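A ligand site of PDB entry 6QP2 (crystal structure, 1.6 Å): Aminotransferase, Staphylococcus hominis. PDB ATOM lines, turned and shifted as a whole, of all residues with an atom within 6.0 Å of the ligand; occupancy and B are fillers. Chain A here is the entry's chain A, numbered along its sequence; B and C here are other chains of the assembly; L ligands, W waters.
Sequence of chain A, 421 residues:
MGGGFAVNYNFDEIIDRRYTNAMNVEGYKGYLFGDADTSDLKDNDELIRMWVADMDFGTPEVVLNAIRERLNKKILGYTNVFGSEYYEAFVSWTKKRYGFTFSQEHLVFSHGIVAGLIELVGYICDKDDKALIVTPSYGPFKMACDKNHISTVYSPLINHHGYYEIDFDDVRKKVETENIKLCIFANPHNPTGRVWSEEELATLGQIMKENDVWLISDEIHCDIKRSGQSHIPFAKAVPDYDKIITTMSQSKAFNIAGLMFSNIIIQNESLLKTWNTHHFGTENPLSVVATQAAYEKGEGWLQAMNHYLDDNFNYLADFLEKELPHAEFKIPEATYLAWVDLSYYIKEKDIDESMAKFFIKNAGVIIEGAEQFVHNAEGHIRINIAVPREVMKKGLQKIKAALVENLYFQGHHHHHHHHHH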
ATOM      1  N   ALA A  53     -27.176  24.108 -19.460  1.00  0.00           N
ATOM      2  CA  ALA A  53     -28.413  23.440 -19.100  1.00  0.00           C
ATOM      3  C   ALA A  53     -28.202  22.307 -18.064  1.00  0.00           C
ATOM      4  O   ALA A  53     -28.360  21.087 -18.376  1.00  0.00           O
ATOM      5  CB  ALA A  53     -29.058  22.955 -20.359  1.00  0.00           C
ATOM      6  N   HIS A 111     -23.548   6.610 -22.581  1.00  0.00           N
ATOM      7  CA  HIS A 111     -23.027   7.442 -21.496  1.00  0.00           C
ATOM      8  C   HIS A 111     -23.356   8.904 -21.811  1.00  0.00           C
ATOM      9  O   HIS A 111     -22.490   9.701 -22.143  1.00  0.00           O
ATOM     10  CB  HIS A 111     -21.530   7.199 -21.306  1.00  0.00           C
ATOM     11  CG  HIS A 111     -21.227   5.787 -20.931  1.00  0.00           C
ATOM     12  ND1 HIS A 111     -20.020   5.178 -21.205  1.00  0.00           N
ATOM     13  CD2 HIS A 111     -22.001   4.842 -20.354  1.00  0.00           C
ATOM     14  CE1 HIS A 111     -20.044   3.934 -20.792  1.00  0.00           C
ATOM     15  NE2 HIS A 111     -21.257   3.701 -20.272  1.00  0.00           N
ATOM     16  N   GLY A 112     -24.639   9.232 -21.724  1.00  0.00           N
ATOM     17  CA  GLY A 112     -25.117  10.525 -22.174  1.00  0.00           C
ATOM     18  C   GLY A 112     -25.655  10.459 -23.604  1.00  0.00           C
ATOM     19  O   GLY A 112     -25.336   9.553 -24.354  1.00  0.00           O
ATOM     20  N   ILE A 113     -26.500  11.434 -23.954  1.00  0.00           N
ATOM     21  CA  ILE A 113     -27.222  11.359 -25.193  1.00  0.00           C
ATOM     22  C   ILE A 113     -26.280  11.698 -26.365  1.00  0.00           C
ATOM     23  O   ILE A 113     -26.341  11.003 -27.384  1.00  0.00           O
ATOM     24  CB  ILE A 113     -28.539  12.153 -25.132  1.00  0.00           C
ATOM     25  CG1 ILE A 113     -29.578  11.306 -24.390  1.00  0.00           C
ATOM     26  CG2 ILE A 113     -28.999  12.542 -26.535  1.00  0.00           C
ATOM     27  CD1 ILE A 113     -30.989  11.812 -24.430  1.00  0.00           C
ATOM     28  N   VAL A 114     -25.406  12.681 -26.198  1.00  0.00           N
ATOM     29  CA  VAL A 114     -24.499  13.086 -27.258  1.00  0.00           C
ATOM     30  C   VAL A 114     -23.527  11.936 -27.578  1.00  0.00           C
ATOM     31  O   VAL A 114     -23.293  11.666 -28.738  1.00  0.00           O
ATOM     32  CB  VAL A 114     -23.766  14.401 -26.965  1.00  0.00           C
ATOM     33  CG1 VAL A 114     -22.671  14.697 -27.969  1.00  0.00           C
ATOM     34  CG2 VAL A 114     -24.758  15.558 -26.913  1.00  0.00           C
ATOM     35  N   ALA A 115     -23.003  11.243 -26.570  1.00  0.00           N
ATOM     36  CA  ALA A 115     -22.176  10.047 -26.811  1.00  0.00           C
ATOM     37  C   ALA A 115     -22.966   9.031 -27.634  1.00  0.00           C
ATOM     38  O   ALA A 115     -22.413   8.383 -28.514  1.00  0.00           O
ATOM     39  CB  ALA A 115     -21.685   9.445 -25.520  1.00  0.00           C
ATOM     40  N   LEU A 117     -25.454   9.744 -29.752  1.00  0.00           N
ATOM     41  CA  LEU A 117     -25.692  10.264 -31.099  1.00  0.00           C
ATOM     42  C   LEU A 117     -24.437  10.054 -31.957  1.00  0.00           C
ATOM     43  O   LEU A 117     -24.531   9.751 -33.153  1.00  0.00           O
ATOM     44  CB  LEU A 117     -26.043  11.757 -31.049  1.00  0.00           C
ATOM     45  CG  LEU A 117     -27.312  12.157 -30.287  1.00  0.00           C
ATOM     46  CD1 LEU A 117     -27.538  13.671 -30.378  1.00  0.00           C
ATOM     47  CD2 LEU A 117     -28.541  11.415 -30.804  1.00  0.00           C
ATOM     48  N   TYR A 138     -29.997  22.557 -30.790  1.00  0.00           N
ATOM     49  CA  TYR A 138     -28.968  22.085 -29.884  1.00  0.00           C
ATOM     50  C   TYR A 138     -27.681  21.808 -30.689  1.00  0.00           C
ATOM     51  O   TYR A 138     -27.700  21.078 -31.685  1.00  0.00           O
ATOM     52  CB  TYR A 138     -29.510  20.849 -29.159  1.00  0.00           C
ATOM     53  CG  TYR A 138     -28.596  20.220 -28.135  1.00  0.00           C
ATOM     54  CD1 TYR A 138     -28.100  20.945 -27.048  1.00  0.00           C
ATOM     55  CD2 TYR A 138     -28.267  18.877 -28.231  1.00  0.00           C
ATOM     56  CE1 TYR A 138     -27.273  20.343 -26.100  1.00  0.00           C
ATOM     57  CE2 TYR A 138     -27.469  18.268 -27.280  1.00  0.00           C
ATOM     58  CZ  TYR A 138     -26.966  18.995 -26.223  1.00  0.00           C
ATOM     59  OH  TYR A 138     -26.165  18.352 -25.322  1.00  0.00           O
ATOM     60  N   PHE A 141     -26.140  18.236 -32.034  1.00  0.00           N
ATOM     61  CA  PHE A 141     -26.721  17.567 -33.210  1.00  0.00           C
ATOM     62  C   PHE A 141     -25.739  17.741 -34.389  1.00  0.00           C
ATOM     63  O   PHE A 141     -25.381  16.785 -35.088  1.00  0.00           O
ATOM     64  CB  PHE A 141     -28.084  18.156 -33.581  1.00  0.00           C
ATOM     65  CG  PHE A 141     -29.218  17.717 -32.696  1.00  0.00           C
ATOM     66  CD1 PHE A 141     -28.992  16.998 -31.535  1.00  0.00           C
ATOM     67  CD2 PHE A 141     -30.523  18.035 -33.041  1.00  0.00           C
ATOM     68  CE1 PHE A 141     -30.060  16.579 -30.756  1.00  0.00           C
ATOM     69  CE2 PHE A 141     -31.583  17.632 -32.248  1.00  0.00           C
ATOM     70  CZ  PHE A 141     -31.348  16.909 -31.109  1.00  0.00           C
ATOM     71  N   ALA A 186     -35.195  17.015 -32.021  1.00  0.00           N
ATOM     72  CA  ALA A 186     -35.468  17.184 -30.580  1.00  0.00           C
ATOM     73  C   ALA A 186     -36.973  17.300 -30.352  1.00  0.00           C
ATOM     74  O   ALA A 186     -37.618  18.171 -30.910  1.00  0.00           O
ATOM     75  CB  ALA A 186     -34.748  18.399 -30.059  1.00  0.00           C
ATOM     76  N   PRO A 188     -39.299  17.164 -26.907  1.00  0.00           N
ATOM     77  CA  PRO A 188     -39.542  18.534 -27.304  1.00  0.00           C
ATOM     78  C   PRO A 188     -38.281  19.270 -27.765  1.00  0.00           C
ATOM     79  O   PRO A 188     -37.158  18.810 -27.516  1.00  0.00           O
ATOM     80  CB  PRO A 188     -40.018  19.256 -26.019  1.00  0.00           C
ATOM     81  CG  PRO A 188     -40.217  18.186 -24.994  1.00  0.00           C
ATOM     82  CD  PRO A 188     -39.529  16.937 -25.491  1.00  0.00           C
ATOM     83  N   ASN A 190     -35.225  22.009 -28.345  1.00  0.00           N
ATOM     84  CA  ASN A 190     -34.286  22.961 -27.730  1.00  0.00           C
ATOM     85  C   ASN A 190     -33.659  23.747 -28.891  1.00  0.00           C
ATOM     86  O   ASN A 190     -33.079  23.120 -29.758  1.00  0.00           O
ATOM     87  CB  ASN A 190     -33.269  22.175 -26.877  1.00  0.00           C
ATOM     88  CG  ASN A 190     -32.084  22.995 -26.397  1.00  0.00           C
ATOM     89  OD1 ASN A 190     -32.123  24.225 -26.462  1.00  0.00           O
ATOM     90  ND2 ASN A 190     -31.071  22.344 -25.861  1.00  0.00           N
ATOM     91  N   ASP A 218     -34.711  12.823 -30.002  1.00  0.00           N
ATOM     92  CA  ASP A 218     -34.081  13.078 -28.736  1.00  0.00           C
ATOM     93  C   ASP A 218     -35.100  13.713 -27.792  1.00  0.00           C
ATOM     94  O   ASP A 218     -35.453  14.878 -27.945  1.00  0.00           O
ATOM     95  CB  ASP A 218     -32.852  13.952 -28.986  1.00  0.00           C
ATOM     96  CG  ASP A 218     -32.100  14.331 -27.740  1.00  0.00           C
ATOM     97  OD1 ASP A 218     -32.563  13.994 -26.634  1.00  0.00           O
ATOM     98  OD2 ASP A 218     -31.015  14.948 -27.892  1.00  0.00           O
ATOM     99  N   ILE A 220     -35.051  14.042 -24.393  1.00  0.00           N
ATOM    100  CA  ILE A 220     -34.501  14.312 -23.069  1.00  0.00           C
ATOM    101  C   ILE A 220     -35.301  15.377 -22.293  1.00  0.00           C
ATOM    102  O   ILE A 220     -35.251  15.356 -21.075  1.00  0.00           O
ATOM    103  CB  ILE A 220     -33.013  14.726 -23.204  1.00  0.00           C
ATOM    104  CG1 ILE A 220     -32.293  14.607 -21.854  1.00  0.00           C
ATOM    105  CG2 ILE A 220     -32.905  16.114 -23.767  1.00  0.00           C
ATOM    106  CD1 ILE A 220     -30.817  14.885 -21.932  1.00  0.00           C
ATOM    107  N   HIS A 221     -36.020  16.292 -22.957  1.00  0.00           N
ATOM    108  CA  HIS A 221     -36.786  17.324 -22.227  1.00  0.00           C
ATOM    109  C   HIS A 221     -38.249  16.896 -21.981  1.00  0.00           C
ATOM    110  O   HIS A 221     -39.058  17.701 -21.499  1.00  0.00           O
ATOM    111  CB  HIS A 221     -36.767  18.654 -22.980  1.00  0.00           C
ATOM    112  CG  HIS A 221     -35.416  19.253 -23.111  1.00  0.00           C
ATOM    113  ND1 HIS A 221     -34.821  19.998 -22.113  1.00  0.00           N
ATOM    114  CD2 HIS A 221     -34.535  19.223 -24.153  1.00  0.00           C
ATOM    115  CE1 HIS A 221     -33.629  20.397 -22.543  1.00  0.00           C
ATOM    116  NE2 HIS A 221     -33.435  19.917 -23.787  1.00  0.00           N
ATOM    117  N   SER A 249     -33.567  10.084 -21.085  1.00  0.00           N
ATOM    118  CA  SER A 249     -32.726  10.066 -19.925  1.00  0.00           C
ATOM    119  C   SER A 249     -33.448  10.764 -18.770  1.00  0.00           C
ATOM    120  O   SER A 249     -34.382  11.517 -19.008  1.00  0.00           O
ATOM    121  CB  SER A 249     -31.420  10.752 -20.278  1.00  0.00           C
ATOM    122  OG  SER A 249     -30.513  10.680 -19.197  1.00  0.00           O
ATOM    123  N   SER A 251     -31.347  12.650 -17.032  1.00  0.00           N
ATOM    124  CA  SER A 251     -30.281  13.654 -16.764  1.00  0.00           C
ATOM    125  C   SER A 251     -30.815  15.078 -16.645  1.00  0.00           C
ATOM    126  O   SER A 251     -30.361  15.751 -15.789  1.00  0.00           O
ATOM    127  CB  SER A 251     -29.179  13.580 -17.767  1.00  0.00           C
ATOM    128  OG  SER A 251     -29.668  13.991 -19.003  1.00  0.00           O
ATOM    129  N   LYS A 252     -31.713  15.493 -17.524  1.00  0.00           N
ATOM    130  CA  LYS A 252     -32.215  16.891 -17.472  1.00  0.00           C
ATOM    131  C   LYS A 252     -33.246  17.058 -16.355  1.00  0.00           C
ATOM    132  O   LYS A 252     -32.992  18.049 -15.573  1.00  0.00           O
ATOM    133  CB  LYS A 252     -32.757  17.331 -18.837  1.00  0.00           C
ATOM    134  CG  LYS A 252     -31.726  17.694 -19.897  1.00  0.00           C
ATOM    135  CD  LYS A 252     -31.315  19.153 -19.873  1.00  0.00           C
ATOM    136  CE  LYS A 252     -30.045  19.505 -20.661  1.00  0.00           C
ATOM    137  NZ  LYS A 252     -29.870  18.662 -21.843  1.00  0.00           N
ATOM    138  N   ALA A 257     -26.968  15.001 -14.993  1.00  0.00           N
ATOM    139  CA  ALA A 257     -26.189  14.968 -16.224  1.00  0.00           C
ATOM    140  C   ALA A 257     -24.788  14.379 -15.985  1.00  0.00           C
ATOM    141  O   ALA A 257     -24.277  13.685 -16.868  1.00  0.00           O
ATOM    142  CB  ALA A 257     -26.046  16.345 -16.868  1.00  0.00           C
ATOM    143  N   SER A 262     -27.956   7.051 -20.269  1.00  0.00           N
ATOM    144  CA  SER A 262     -29.017   7.406 -21.166  1.00  0.00           C
ATOM    145  C   SER A 262     -29.603   6.130 -21.738  1.00  0.00           C
ATOM    146  O   SER A 262     -28.852   5.193 -21.996  1.00  0.00           O
ATOM    147  CB  SER A 262     -28.543   8.265 -22.330  1.00  0.00           C
ATOM    148  OG  SER A 262     -27.564   9.206 -21.948  1.00  0.00           O
ATOM    149  N   LEU A 337     -35.768  26.427 -20.375  1.00  0.00           N
ATOM    150  CA  LEU A 337     -34.937  27.349 -21.143  1.00  0.00           C
ATOM    151  C   LEU A 337     -35.829  28.350 -21.880  1.00  0.00           C
ATOM    152  O   LEU A 337     -36.792  27.940 -22.549  1.00  0.00           O
ATOM    153  CB  LEU A 337     -34.140  26.503 -22.137  1.00  0.00           C
ATOM    154  CG  LEU A 337     -33.252  25.432 -21.501  1.00  0.00           C
ATOM    155  CD1 LEU A 337     -32.857  24.396 -22.517  1.00  0.00           C
ATOM    156  CD2 LEU A 337     -32.047  26.015 -20.784  1.00  0.00           C
ATOM    157  N   ARG A 382     -30.543  32.431 -24.996  1.00  0.00           N
ATOM    158  CA  ARG A 382     -31.241  31.425 -24.229  1.00  0.00           C
ATOM    159  C   ARG A 382     -30.897  31.588 -22.749  1.00  0.00           C
ATOM    160  O   ARG A 382     -29.693  31.615 -22.353  1.00  0.00           O
ATOM    161  CB  ARG A 382     -30.860  30.037 -24.730  1.00  0.00           C
ATOM    162  CG  ARG A 382     -31.856  28.965 -24.294  1.00  0.00           C
ATOM    163  CD  ARG A 382     -31.328  27.551 -24.534  1.00  0.00           C
ATOM    164  NE  ARG A 382     -30.223  27.236 -23.627  1.00  0.00           N
ATOM    165  CZ  ARG A 382     -29.550  26.095 -23.622  1.00  0.00           C
ATOM    166  NH1 ARG A 382     -28.580  25.893 -22.741  1.00  0.00           N
ATOM    167  NH2 ARG A 382     -29.871  25.134 -24.482  1.00  0.00           N
ATOM    168  N   TYR B  78     -23.119  18.850 -14.891  1.00  0.00           N
ATOM    169  CA  TYR B  78     -22.042  18.732 -15.842  1.00  0.00           C
ATOM    170  C   TYR B  78     -20.729  19.042 -15.134  1.00  0.00           C
ATOM    171  O   TYR B  78     -20.597  20.043 -14.402  1.00  0.00           O
ATOM    172  CB  TYR B  78     -22.280  19.654 -17.041  1.00  0.00           C
ATOM    173  CG  TYR B  78     -23.320  19.135 -18.002  1.00  0.00           C
ATOM    174  CD1 TYR B  78     -23.074  18.009 -18.777  1.00  0.00           C
ATOM    175  CD2 TYR B  78     -24.551  19.760 -18.117  1.00  0.00           C
ATOM    176  CE1 TYR B  78     -24.032  17.529 -19.653  1.00  0.00           C
ATOM    177  CE2 TYR B  78     -25.520  19.284 -18.985  1.00  0.00           C
ATOM    178  CZ  TYR B  78     -25.259  18.177 -19.775  1.00  0.00           C
ATOM    179  OH  TYR B  78     -26.242  17.696 -20.599  1.00  0.00           O
ATOM    180  N   HIS C   3     -19.373  20.736 -24.171  1.00  0.00           N
ATOM    181  CA  HIS C   3     -19.645  20.036 -25.431  1.00  0.00           C
ATOM    182  C   HIS C   3     -20.945  20.535 -26.095  1.00  0.00           C
ATOM    183  O   HIS C   3     -21.109  20.316 -27.282  1.00  0.00           O
ATOM    184  CB  HIS C   3     -19.614  18.514 -25.234  1.00  0.00           C
ATOM    185  CG  HIS C   3     -20.816  17.915 -24.578  1.00  0.00           C
ATOM    186  ND1 HIS C   3     -20.950  17.836 -23.192  1.00  0.00           N
ATOM    187  CD2 HIS C   3     -21.914  17.315 -25.100  1.00  0.00           C
ATOM    188  CE1 HIS C   3     -22.072  17.219 -22.893  1.00  0.00           C
ATOM    189  NE2 HIS C   3     -22.692  16.889 -24.047  1.00  0.00           N
ATOM    190  N   HIS C   4     -21.829  21.217 -25.342  1.00  0.00           N
ATOM    191  CA  HIS C   4     -23.009  21.894 -25.924  1.00  0.00           C
ATOM    192  C   HIS C   4     -22.587  23.093 -26.793  1.00  0.00           C
ATOM    193  O   HIS C   4     -23.381  23.574 -27.611  1.00  0.00           O
ATOM    194  CB  HIS C   4     -24.020  22.344 -24.848  1.00  0.00           C
ATOM    195  CG  HIS C   4     -24.627  21.241 -24.035  1.00  0.00           C
ATOM    196  ND1 HIS C   4     -25.754  21.448 -23.256  1.00  0.00           N
ATOM    197  CD2 HIS C   4     -24.281  19.949 -23.862  1.00  0.00           C
ATOM    198  CE1 HIS C   4     -26.076  20.321 -22.645  1.00  0.00           C
ATOM    199  NE2 HIS C   4     -25.190  19.383 -22.996  1.00  0.00           N
HETATM  200  N1  LIG L   1     -30.179  16.568 -26.212  1.00  0.00           N
HETATM  201  C1  LIG L   1     -30.801  17.734 -26.164  1.00  0.00           C
HETATM  202  C2  LIG L   1     -31.781  18.064 -27.234  1.00  0.00           C
HETATM  203  C3  LIG L   1     -30.573  18.606 -25.111  1.00  0.00           C
HETATM  204  O1  LIG L   1     -31.239  19.757 -25.123  1.00  0.00           O
HETATM  205  C4  LIG L   1     -29.644  18.282 -24.120  1.00  0.00           C
HETATM  206  C5  LIG L   1     -29.445  19.113 -22.950  1.00  0.00           C
HETATM  207  C6  LIG L   1     -28.998  17.043 -24.207  1.00  0.00           C
HETATM  208  C7  LIG L   1     -29.286  16.244 -25.267  1.00  0.00           C
HETATM  209  C8  LIG L   1     -28.012  16.585 -23.182  1.00  0.00           C
HETATM  210  O2  LIG L   1     -27.054  15.668 -23.789  1.00  0.00           O
HETATM  211  P1  LIG L   1     -25.936  14.966 -22.959  1.00  0.00           P
HETATM  212  O3  LIG L   1     -24.968  14.450 -23.910  1.00  0.00           O
HETATM  213  O4  LIG L   1     -25.392  16.001 -22.072  1.00  0.00           O
HETATM  214  O5  LIG L   1     -26.599  13.940 -22.210  1.00  0.00           O
HETATM  215  O   HOH W   1     -22.983  12.436 -24.003  1.00  0.00           O
HETATM  216  O   HOH W   2     -25.152  13.019 -19.357  1.00  0.00           O
HETATM  217  O   HOH W   3     -28.437  12.054 -21.054  1.00  0.00           O
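A ring nitrogen (NE2) of His 221 lies within hydrogen-bond range of an oxygen (O1) of the ligand.
O1 of the ligand sits at hydrogen-bond distance from ND2 of Asn 190 (2.7 Å).
N of Ile 113 is in hydrogen-bond range of O5 of the ligand (3.1 Å).
The side-chain carboxylate (OD2) of Asp 218 is in hydrogen-bond range of a nitrogen (N1) of the ligand, 2.5 Å away.
The side-chain hydroxyl (OH) of Tyr 138 sits at hydrogen-bond distance from an oxygen (O2) of the ligand (3.2 Å).
NE2 of His 3 of chain C sits at hydrogen-bond distance from O3 of the ligand.
An oxygen (O3) of the ligand lies within hydrogen-bond range of the backbone NH (N) of Val 114, 2.9 Å away.
NZ of Lys 252 is bonded to C5 of the ligand (1.3 Å).
An oxygen (O4) of the ligand is in hydrogen-bond range of the side-chain hydroxyl (OH) of Tyr 78 of chain B, 2.4 Å away.
The side-chain amide oxygen (OD1) of Asn 190 sits at hydrogen-bond distance from the guanidinium group (NH2) of Arg 382.
N of Ile 220 sits at hydrogen-bond distance from OD1 of Asp 218, 3.3 Å away.
The side-chain hydroxyl (OG) of Ser 262 is in hydrogen-bond range of the backbone NH (N) of Ile 113 (3.2 Å).
The backbone NH (N) of Tyr 138 lies within hydrogen-bond range of the backbone carbonyl oxygen (O) of Asn 190, at 3.3 Å.
The backbone NH (N) of Gly 112 sits close to the side-chain hydroxyl (OG) of Ser 262 (2.9 Å).
NE2 of His 4 of chain C lies within hydrogen-bond range of OH of Tyr 78 of chain B, 3.1 Å away.
OH of Tyr 138 lies within hydrogen-bond range of NE2 of His 4 of chain C (2.7 Å).
Gly 112 touches the ligand (CA to O5, 3.7 Å).
Ile 220 touches the ligand (CD1 to C8, 3.5 Å).
NE2 of His 4 of chain C touches O4 of the ligand, at 3.5 Å.
Hydrophobic or aromatic side chains within 4 Å of the ligand: Ile 113, Val 114, Tyr 138, Ile 220, His 221, Tyr 78 of chain B, His 3 of chain C and His 4 of chain C.
Within 4 Å of the ligand: Gly 112, Ile 113, Val 114, Tyr 138, Asn 190, Asp 218, Ile 220, His 221, Lys 252, Tyr 78 of chain B, His 3 of chain C and His 4 of chain C.
Along chain A the residues within 4 Å of the ligand span positions 112 to 252.
Water W1 lies within hydrogen-bond range of O3 of the ligand, N of Ala 115, N of Val 114 and O of His 111.
Water W3 lies within hydrogen-bond range of an oxygen (O5) of the ligand (2.9 Å), the side-chain hydroxyl (OG) of Ser 251 (3.1 Å), the side-chain hydroxyl (OG) of Ser 249 (3.1 Å) and the side-chain hydroxyl (OG) of Ser 262 (3.1 Å).
Water W2 bridges the backbone carbonyl oxygen (O) of Ala 257 (2.7 Å) and an oxygen (O5) of the ligand (3.3 Å).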
